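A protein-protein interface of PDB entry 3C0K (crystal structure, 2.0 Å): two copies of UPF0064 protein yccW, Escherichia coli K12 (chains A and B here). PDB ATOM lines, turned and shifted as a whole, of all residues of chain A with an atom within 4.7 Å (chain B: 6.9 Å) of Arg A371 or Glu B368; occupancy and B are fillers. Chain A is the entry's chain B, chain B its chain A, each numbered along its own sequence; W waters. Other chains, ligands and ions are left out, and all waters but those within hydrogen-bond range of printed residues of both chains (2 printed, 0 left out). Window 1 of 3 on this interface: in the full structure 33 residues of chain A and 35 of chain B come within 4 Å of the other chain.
The backbone carbonyl oxygen (O) of Val A378 lies within hydrogen-bond range of the backbone NH (N) of Phe B366 (2.8 Å).
The backbone carbonyl oxygen of Phe B366 is in hydrogen-bond range of the guanidinium group of Arg A371 (3.0 Å).
Gln B369 touches its own counterpart, Gln A369.
Printed residues of chain B that touch a printed residue of chain A: Gln B365, Phe B366, Ile B367, Glu B368 and Gln B369.
Hydrophobic or aromatic side chains of chain A within 4 Å of the printed part of chain B: Val A378.
The backbone carbonyl oxygen (O) of Glu B368 is in hydrogen-bond range of the backbone NH (N) of Ala B392 (3.0 Å).
N of Ile B367 is in hydrogen-bond range of O of Ala B392, 3.1 Å away.
The side-chain carboxylate (OE1) of Glu B368 is in hydrogen-bond range of the side-chain hydroxyl (OH) of Tyr B218 (2.6 Å).
Among the printed residues, pairs that only touch across the chains: Val A378 with Gln B365, Gln A369 with Gln B369, Arg A371 with Ile B367 and Arg A371 with Glu B368.
Printed residues of chain B within 4 Å of Arg A371: Phe B366 (3.0 Å), Ile B367 (3.8 Å) and Glu B368 (3.9 Å).
Printed residues of chain B within 4 Å of Val A378: Gln B365 and Phe B366.
Leu B336 touches none of the printed residues of chain A.
Of the printed residues of chain A, Gln B365 touches Val A378 (3.6 Å).
Of the printed residues of chain A, Ile B367 touches Arg A371 (3.8 Å).
Of chain A, only Arg A371 (3.9 Å) comes within 4 Å of Glu B368.
Of the printed residues of chain A, Gln B369 touches Gln A369.
Water W2 lies within hydrogen-bond range of OE1 of Gln B369 (2.6 Å) and NH1 of Arg A371 (3.0 Å).
Water W1 bridges O of Gln A369 (2.8 Å) and O of Gln B369 (3.5 Å).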
ATOM      1  N   ASP A 207     -16.058  16.410  32.312  1.00  0.00           N
ATOM      2  CA  ASP A 207     -14.617  16.370  32.096  1.00  0.00           C
ATOM      3  C   ASP A 207     -14.140  15.560  30.890  1.00  0.00           C
ATOM      4  O   ASP A 207     -13.048  15.799  30.374  1.00  0.00           O
ATOM      5  CB  ASP A 207     -13.897  15.879  33.358  1.00  0.00           C
ATOM      6  CG  ASP A 207     -14.362  14.506  33.818  1.00  0.00           C
ATOM      7  OD1 ASP A 207     -14.992  13.765  33.029  1.00  0.00           O
ATOM      8  OD2 ASP A 207     -14.078  14.161  34.984  1.00  0.00           O
ATOM      9  N   GLN A 369      -2.551  12.243  24.011  1.00  0.00           N
ATOM     10  CA  GLN A 369      -2.698  12.231  25.459  1.00  0.00           C
ATOM     11  C   GLN A 369      -3.906  13.101  25.753  1.00  0.00           C
ATOM     12  O   GLN A 369      -3.987  14.234  25.285  1.00  0.00           O
ATOM     13  CB  GLN A 369      -1.456  12.812  26.148  1.00  0.00           C
ATOM     14  CG  GLN A 369      -1.590  12.938  27.659  1.00  0.00           C
ATOM     15  CD  GLN A 369      -0.263  13.234  28.348  1.00  0.00           C
ATOM     16  OE1 GLN A 369       0.443  14.177  27.987  1.00  0.00           O
ATOM     17  NE2 GLN A 369       0.077  12.428  29.349  1.00  0.00           N
ATOM     18  N   PHE A 370      -4.849  12.563  26.516  1.00  0.00           N
ATOM     19  CA  PHE A 370      -6.055  13.300  26.843  1.00  0.00           C
ATOM     20  C   PHE A 370      -5.932  14.008  28.186  1.00  0.00           C
ATOM     21  O   PHE A 370      -5.069  13.677  28.999  1.00  0.00           O
ATOM     22  CB  PHE A 370      -7.251  12.346  26.826  1.00  0.00           C
ATOM     23  CG  PHE A 370      -7.458  11.677  25.492  1.00  0.00           C
ATOM     24  CD1 PHE A 370      -7.764  12.436  24.361  1.00  0.00           C
ATOM     25  CD2 PHE A 370      -7.316  10.298  25.356  1.00  0.00           C
ATOM     26  CE1 PHE A 370      -7.925  11.831  23.111  1.00  0.00           C
ATOM     27  CE2 PHE A 370      -7.475   9.679  24.108  1.00  0.00           C
ATOM     28  CZ  PHE A 370      -7.779  10.450  22.985  1.00  0.00           C
ATOM     29  N   ARG A 371      -6.801  14.989  28.400  1.00  0.00           N
ATOM     30  CA  ARG A 371      -6.796  15.783  29.621  1.00  0.00           C
ATOM     31  C   ARG A 371      -8.227  16.183  29.949  1.00  0.00           C
ATOM     32  O   ARG A 371      -9.081  16.236  29.060  1.00  0.00           O
ATOM     33  CB  ARG A 371      -5.961  17.047  29.396  1.00  0.00           C
ATOM     34  CG  ARG A 371      -5.870  17.992  30.579  1.00  0.00           C
ATOM     35  CD  ARG A 371      -5.468  19.387  30.120  1.00  0.00           C
ATOM     36  NE  ARG A 371      -5.281  20.311  31.235  1.00  0.00           N
ATOM     37  CZ  ARG A 371      -4.194  20.347  31.996  1.00  0.00           C
ATOM     38  NH1 ARG A 371      -3.184  19.512  31.763  1.00  0.00           N
ATOM     39  NH2 ARG A 371      -4.116  21.212  32.998  1.00  0.00           N
ATOM     40  N   GLN A 372      -8.488  16.464  31.221  1.00  0.00           N
ATOM     41  CA  GLN A 372      -9.818  16.892  31.626  1.00  0.00           C
ATOM     42  C   GLN A 372     -10.114  18.156  30.820  1.00  0.00           C
ATOM     43  O   GLN A 372      -9.201  18.926  30.515  1.00  0.00           O
ATOM     44  CB  GLN A 372      -9.848  17.168  33.133  1.00  0.00           C
ATOM     45  CG  GLN A 372      -8.751  18.110  33.628  1.00  0.00           C
ATOM     46  CD  GLN A 372      -8.336  17.790  35.053  1.00  0.00           C
ATOM     47  OE1 GLN A 372      -7.867  16.688  35.333  1.00  0.00           O
ATOM     48  NE2 GLN A 372      -8.509  18.747  35.959  1.00  0.00           N
ATOM     49  N   ALA A 373     -11.379  18.356  30.457  1.00  0.00           N
ATOM     50  CA  ALA A 373     -11.784  19.516  29.660  1.00  0.00           C
ATOM     51  C   ALA A 373     -11.415  20.866  30.280  1.00  0.00           C
ATOM     52  O   ALA A 373     -11.191  20.970  31.486  1.00  0.00           O
ATOM     53  CB  ALA A 373     -13.293  19.455  29.378  1.00  0.00           C
ATOM     54  N   VAL A 378      -6.582  23.690  35.732  1.00  0.00           N
ATOM     55  CA  VAL A 378      -5.700  23.343  36.836  1.00  0.00           C
ATOM     56  C   VAL A 378      -4.846  24.577  37.118  1.00  0.00           C
ATOM     57  O   VAL A 378      -3.980  24.932  36.312  1.00  0.00           O
ATOM     58  CB  VAL A 378      -4.764  22.173  36.488  1.00  0.00           C
ATOM     59  CG1 VAL A 378      -3.776  21.933  37.652  1.00  0.00           C
ATOM     60  CG2 VAL A 378      -5.574  20.922  36.229  1.00  0.00           C
ATOM     61  N   LEU A 386      -4.785  18.080  38.454  1.00  0.00           N
ATOM     62  CA  LEU A 386      -4.877  17.271  37.243  1.00  0.00           C
ATOM     63  C   LEU A 386      -5.126  15.831  37.679  1.00  0.00           C
ATOM     64  O   LEU A 386      -4.209  15.154  38.148  1.00  0.00           O
ATOM     65  CB  LEU A 386      -3.571  17.364  36.454  1.00  0.00           C
ATOM     66  CG  LEU A 386      -3.558  16.805  35.031  1.00  0.00           C
ATOM     67  CD1 LEU A 386      -4.544  17.580  34.170  1.00  0.00           C
ATOM     68  CD2 LEU A 386      -2.148  16.915  34.453  1.00  0.00           C
ATOM     69  N   LEU A 388      -7.510  13.556  35.712  1.00  0.00           N
ATOM     70  CA  LEU A 388      -7.879  12.713  34.584  1.00  0.00           C
ATOM     71  C   LEU A 388      -6.689  12.375  33.692  1.00  0.00           C
ATOM     72  O   LEU A 388      -6.031  13.259  33.132  1.00  0.00           O
ATOM     73  CB  LEU A 388      -8.995  13.383  33.770  1.00  0.00           C
ATOM     74  CG  LEU A 388      -9.656  12.544  32.668  1.00  0.00           C
ATOM     75  CD1 LEU A 388     -10.997  13.161  32.296  1.00  0.00           C
ATOM     76  CD2 LEU A 388      -8.731  12.449  31.455  1.00  0.00           C
ATOM     77  N   ASP B 210      -0.370  20.168  15.460  1.00  0.00           N
ATOM     78  CA  ASP B 210      -1.482  20.332  16.390  1.00  0.00           C
ATOM     79  C   ASP B 210      -1.396  21.602  17.236  1.00  0.00           C
ATOM     80  O   ASP B 210      -2.416  22.105  17.709  1.00  0.00           O
ATOM     81  CB  ASP B 210      -1.606  19.093  17.279  1.00  0.00           C
ATOM     82  CG  ASP B 210      -2.056  17.865  16.496  1.00  0.00           C
ATOM     83  OD1 ASP B 210      -3.085  17.958  15.789  1.00  0.00           O
ATOM     84  OD2 ASP B 210      -1.392  16.814  16.585  1.00  0.00           O
ATOM     85  N   ALA B 214      -4.428  24.343  17.376  1.00  0.00           N
ATOM     86  CA  ALA B 214      -4.964  24.875  18.625  1.00  0.00           C
ATOM     87  C   ALA B 214      -4.888  26.402  18.665  1.00  0.00           C
ATOM     88  O   ALA B 214      -5.723  27.058  19.284  1.00  0.00           O
ATOM     89  CB  ALA B 214      -4.210  24.285  19.801  1.00  0.00           C
ATOM     90  N   THR B 215      -3.876  26.972  18.020  1.00  0.00           N
ATOM     91  CA  THR B 215      -3.750  28.423  18.006  1.00  0.00           C
ATOM     92  C   THR B 215      -5.015  29.023  17.389  1.00  0.00           C
ATOM     93  O   THR B 215      -5.495  30.071  17.824  1.00  0.00           O
ATOM     94  CB  THR B 215      -2.505  28.873  17.200  1.00  0.00           C
ATOM     95  OG1 THR B 215      -1.318  28.378  17.835  1.00  0.00           O
ATOM     96  CG2 THR B 215      -2.430  30.396  17.129  1.00  0.00           C
ATOM     97  N   ARG B 217      -8.089  28.031  17.598  1.00  0.00           N
ATOM     98  CA  ARG B 217      -9.221  28.010  18.512  1.00  0.00           C
ATOM     99  C   ARG B 217      -9.325  29.233  19.413  1.00  0.00           C
ATOM    100  O   ARG B 217     -10.418  29.711  19.690  1.00  0.00           O
ATOM    101  CB  ARG B 217      -9.160  26.743  19.376  1.00  0.00           C
ATOM    102  CG  ARG B 217     -10.316  26.578  20.356  1.00  0.00           C
ATOM    103  CD  ARG B 217     -10.868  25.144  20.343  1.00  0.00           C
ATOM    104  NE  ARG B 217     -11.784  24.883  21.457  1.00  0.00           N
ATOM    105  CZ  ARG B 217     -11.432  25.006  22.732  1.00  0.00           C
ATOM    106  NH1 ARG B 217     -10.197  25.382  23.034  1.00  0.00           N
ATOM    107  NH2 ARG B 217     -12.301  24.752  23.700  1.00  0.00           N
ATOM    108  N   TYR B 218      -8.183  29.752  19.837  1.00  0.00           N
ATOM    109  CA  TYR B 218      -8.145  30.873  20.771  1.00  0.00           C
ATOM    110  C   TYR B 218      -8.114  32.297  20.241  1.00  0.00           C
ATOM    111  O   TYR B 218      -8.324  33.233  21.006  1.00  0.00           O
ATOM    112  CB  TYR B 218      -6.929  30.703  21.681  1.00  0.00           C
ATOM    113  CG  TYR B 218      -6.936  29.426  22.479  1.00  0.00           C
ATOM    114  CD1 TYR B 218      -7.739  29.299  23.606  1.00  0.00           C
ATOM    115  CD2 TYR B 218      -6.141  28.343  22.108  1.00  0.00           C
ATOM    116  CE1 TYR B 218      -7.751  28.133  24.351  1.00  0.00           C
ATOM    117  CE2 TYR B 218      -6.148  27.169  22.843  1.00  0.00           C
ATOM    118  CZ  TYR B 218      -6.955  27.073  23.968  1.00  0.00           C
ATOM    119  OH  TYR B 218      -6.960  25.930  24.723  1.00  0.00           O
ATOM    120  N   LEU B 336       0.317  30.303  24.829  1.00  0.00           N
ATOM    121  CA  LEU B 336       0.568  29.004  24.221  1.00  0.00           C
ATOM    122  C   LEU B 336       2.086  28.985  24.224  1.00  0.00           C
ATOM    123  O   LEU B 336       2.725  29.684  23.430  1.00  0.00           O
ATOM    124  CB  LEU B 336       0.015  28.968  22.794  1.00  0.00           C
ATOM    125  CG  LEU B 336      -1.469  29.350  22.683  1.00  0.00           C
ATOM    126  CD1 LEU B 336      -1.906  29.372  21.223  1.00  0.00           C
ATOM    127  CD2 LEU B 336      -2.303  28.362  23.476  1.00  0.00           C
ATOM    128  N   GLN B 350       6.312  22.589  33.446  1.00  0.00           N
ATOM    129  CA  GLN B 350       5.152  23.084  34.186  1.00  0.00           C
ATOM    130  C   GLN B 350       5.619  23.893  35.386  1.00  0.00           C
ATOM    131  O   GLN B 350       5.062  24.947  35.688  1.00  0.00           O
ATOM    132  CB  GLN B 350       4.284  21.933  34.695  1.00  0.00           C
ATOM    133  CG  GLN B 350       3.781  21.009  33.626  1.00  0.00           C
ATOM    134  CD  GLN B 350       2.809  19.976  34.162  1.00  0.00           C
ATOM    135  OE1 GLN B 350       1.812  20.322  34.798  1.00  0.00           O
ATOM    136  NE2 GLN B 350       3.093  18.701  33.902  1.00  0.00           N
ATOM    137  N   GLN B 365      -3.908  29.404  34.779  1.00  0.00           N
ATOM    138  CA  GLN B 365      -4.577  28.113  34.779  1.00  0.00           C
ATOM    139  C   GLN B 365      -4.113  27.312  33.572  1.00  0.00           C
ATOM    140  O   GLN B 365      -4.081  27.829  32.461  1.00  0.00           O
ATOM    141  CB  GLN B 365      -6.092  28.285  34.657  1.00  0.00           C
ATOM    142  CG  GLN B 365      -6.770  29.106  35.731  1.00  0.00           C
ATOM    143  CD  GLN B 365      -8.221  29.377  35.378  1.00  0.00           C
ATOM    144  OE1 GLN B 365      -8.521  29.832  34.273  1.00  0.00           O
ATOM    145  NE2 GLN B 365      -9.125  29.103  36.311  1.00  0.00           N
ATOM    146  N   PHE B 366      -3.748  26.055  33.788  1.00  0.00           N
ATOM    147  CA  PHE B 366      -3.367  25.196  32.679  1.00  0.00           C
ATOM    148  C   PHE B 366      -4.690  24.602  32.198  1.00  0.00           C
ATOM    149  O   PHE B 366      -5.378  23.912  32.951  1.00  0.00           O
ATOM    150  CB  PHE B 366      -2.426  24.094  33.154  1.00  0.00           C
ATOM    151  CG  PHE B 366      -1.049  24.583  33.484  1.00  0.00           C
ATOM    152  CD1 PHE B 366      -0.242  25.143  32.495  1.00  0.00           C
ATOM    153  CD2 PHE B 366      -0.550  24.484  34.781  1.00  0.00           C
ATOM    154  CE1 PHE B 366       1.048  25.596  32.793  1.00  0.00           C
ATOM    155  CE2 PHE B 366       0.739  24.934  35.089  1.00  0.00           C
ATOM    156  CZ  PHE B 366       1.536  25.488  34.099  1.00  0.00           C
ATOM    157  N   ILE B 367      -5.054  24.886  30.953  1.00  0.00           N
ATOM    158  CA  ILE B 367      -6.317  24.404  30.402  1.00  0.00           C
ATOM    159  C   ILE B 367      -6.135  23.407  29.264  1.00  0.00           C
ATOM    160  O   ILE B 367      -7.095  22.774  28.819  1.00  0.00           O
ATOM    161  CB  ILE B 367      -7.167  25.582  29.881  1.00  0.00           C
ATOM    162  CG1 ILE B 367      -6.352  26.413  28.883  1.00  0.00           C
ATOM    163  CG2 ILE B 367      -7.614  26.449  31.039  1.00  0.00           C
ATOM    164  CD1 ILE B 367      -7.131  27.551  28.230  1.00  0.00           C
ATOM    165  N   GLU B 368      -4.907  23.269  28.790  1.00  0.00           N
ATOM    166  CA  GLU B 368      -4.637  22.351  27.703  1.00  0.00           C
ATOM    167  C   GLU B 368      -3.151  22.020  27.667  1.00  0.00           C
ATOM    168  O   GLU B 368      -2.312  22.837  28.051  1.00  0.00           O
ATOM    169  CB  GLU B 368      -5.109  22.978  26.382  1.00  0.00           C
ATOM    170  CG  GLU B 368      -4.774  22.188  25.138  1.00  0.00           C
ATOM    171  CD  GLU B 368      -5.447  22.749  23.892  1.00  0.00           C
ATOM    172  OE1 GLU B 368      -5.550  23.992  23.765  1.00  0.00           O
ATOM    173  OE2 GLU B 368      -5.860  21.943  23.032  1.00  0.00           O
ATOM    174  N   GLN B 369      -2.837  20.803  27.235  1.00  0.00           N
ATOM    175  CA  GLN B 369      -1.458  20.342  27.147  1.00  0.00           C
ATOM    176  C   GLN B 369      -1.195  19.858  25.725  1.00  0.00           C
ATOM    177  O   GLN B 369      -1.998  19.119  25.156  1.00  0.00           O
ATOM    178  CB  GLN B 369      -1.224  19.217  28.162  1.00  0.00           C
ATOM    179  CG  GLN B 369       0.152  18.558  28.098  1.00  0.00           C
ATOM    180  CD  GLN B 369       0.463  17.752  29.351  1.00  0.00           C
ATOM    181  OE1 GLN B 369      -0.436  17.196  29.980  1.00  0.00           O
ATOM    182  NE2 GLN B 369       1.740  17.679  29.711  1.00  0.00           N
ATOM    183  N   PHE B 370      -0.074  20.286  25.150  1.00  0.00           N
ATOM    184  CA  PHE B 370       0.274  19.913  23.781  1.00  0.00           C
ATOM    185  C   PHE B 370       1.410  18.901  23.704  1.00  0.00           C
ATOM    186  O   PHE B 370       2.174  18.729  24.653  1.00  0.00           O
ATOM    187  CB  PHE B 370       0.674  21.161  22.982  1.00  0.00           C
ATOM    188  CG  PHE B 370      -0.335  22.265  23.039  1.00  0.00           C
ATOM    189  CD1 PHE B 370      -1.612  22.085  22.525  1.00  0.00           C
ATOM    190  CD2 PHE B 370      -0.012  23.487  23.622  1.00  0.00           C
ATOM    191  CE1 PHE B 370      -2.559  23.110  22.590  1.00  0.00           C
ATOM    192  CE2 PHE B 370      -0.950  24.516  23.691  1.00  0.00           C
ATOM    193  CZ  PHE B 370      -2.227  24.326  23.173  1.00  0.00           C
ATOM    194  N   GLY B 390       4.301  21.323  25.689  1.00  0.00           N
ATOM    195  CA  GLY B 390       3.622  22.591  25.505  1.00  0.00           C
ATOM    196  C   GLY B 390       2.380  22.729  26.358  1.00  0.00           C
ATOM    197  O   GLY B 390       1.770  21.731  26.749  1.00  0.00           O
ATOM    198  N   PHE B 391       2.001  23.972  26.639  1.00  0.00           N
ATOM    199  CA  PHE B 391       0.821  24.243  27.447  1.00  0.00           C
ATOM    200  C   PHE B 391       0.076  25.481  26.987  1.00  0.00           C
ATOM    201  O   PHE B 391       0.664  26.407  26.428  1.00  0.00           O
ATOM    202  CB  PHE B 391       1.211  24.456  28.913  1.00  0.00           C
ATOM    203  CG  PHE B 391       1.620  23.207  29.621  1.00  0.00           C
ATOM    204  CD1 PHE B 391       0.667  22.276  30.017  1.00  0.00           C
ATOM    205  CD2 PHE B 391       2.960  22.951  29.881  1.00  0.00           C
ATOM    206  CE1 PHE B 391       1.041  21.103  30.663  1.00  0.00           C
ATOM    207  CE2 PHE B 391       3.345  21.782  30.526  1.00  0.00           C
ATOM    208  CZ  PHE B 391       2.379  20.856  30.918  1.00  0.00           C
ATOM    209  N   ALA B 392      -1.227  25.476  27.233  1.00  0.00           N
ATOM    210  CA  ALA B 392      -2.079  26.619  26.942  1.00  0.00           C
ATOM    211  C   ALA B 392      -2.379  27.087  28.362  1.00  0.00           C
ATOM    212  O   ALA B 392      -2.942  26.326  29.152  1.00  0.00           O
ATOM    213  CB  ALA B 392      -3.356  26.175  26.247  1.00  0.00           C
ATOM    214  N   CYS B 393      -1.985  28.316  28.688  1.00  0.00           N
ATOM    215  CA  CYS B 393      -2.187  28.864  30.028  1.00  0.00           C
ATOM    216  C   CYS B 393      -3.068  30.102  30.014  1.00  0.00           C
ATOM    217  O   CYS B 393      -2.832  31.032  29.242  1.00  0.00           O
ATOM    218  CB  CYS B 393      -0.834  29.224  30.646  1.00  0.00           C
ATOM    219  SG  CYS B 393       0.441  28.006  30.300  1.00  0.00           S
HETATM  220  O   HOH W   1      -3.100  16.320  26.871  1.00  0.00           O
HETATM  221  O   HOH W   2      -3.004  17.115  30.027  1.00  0.00           O
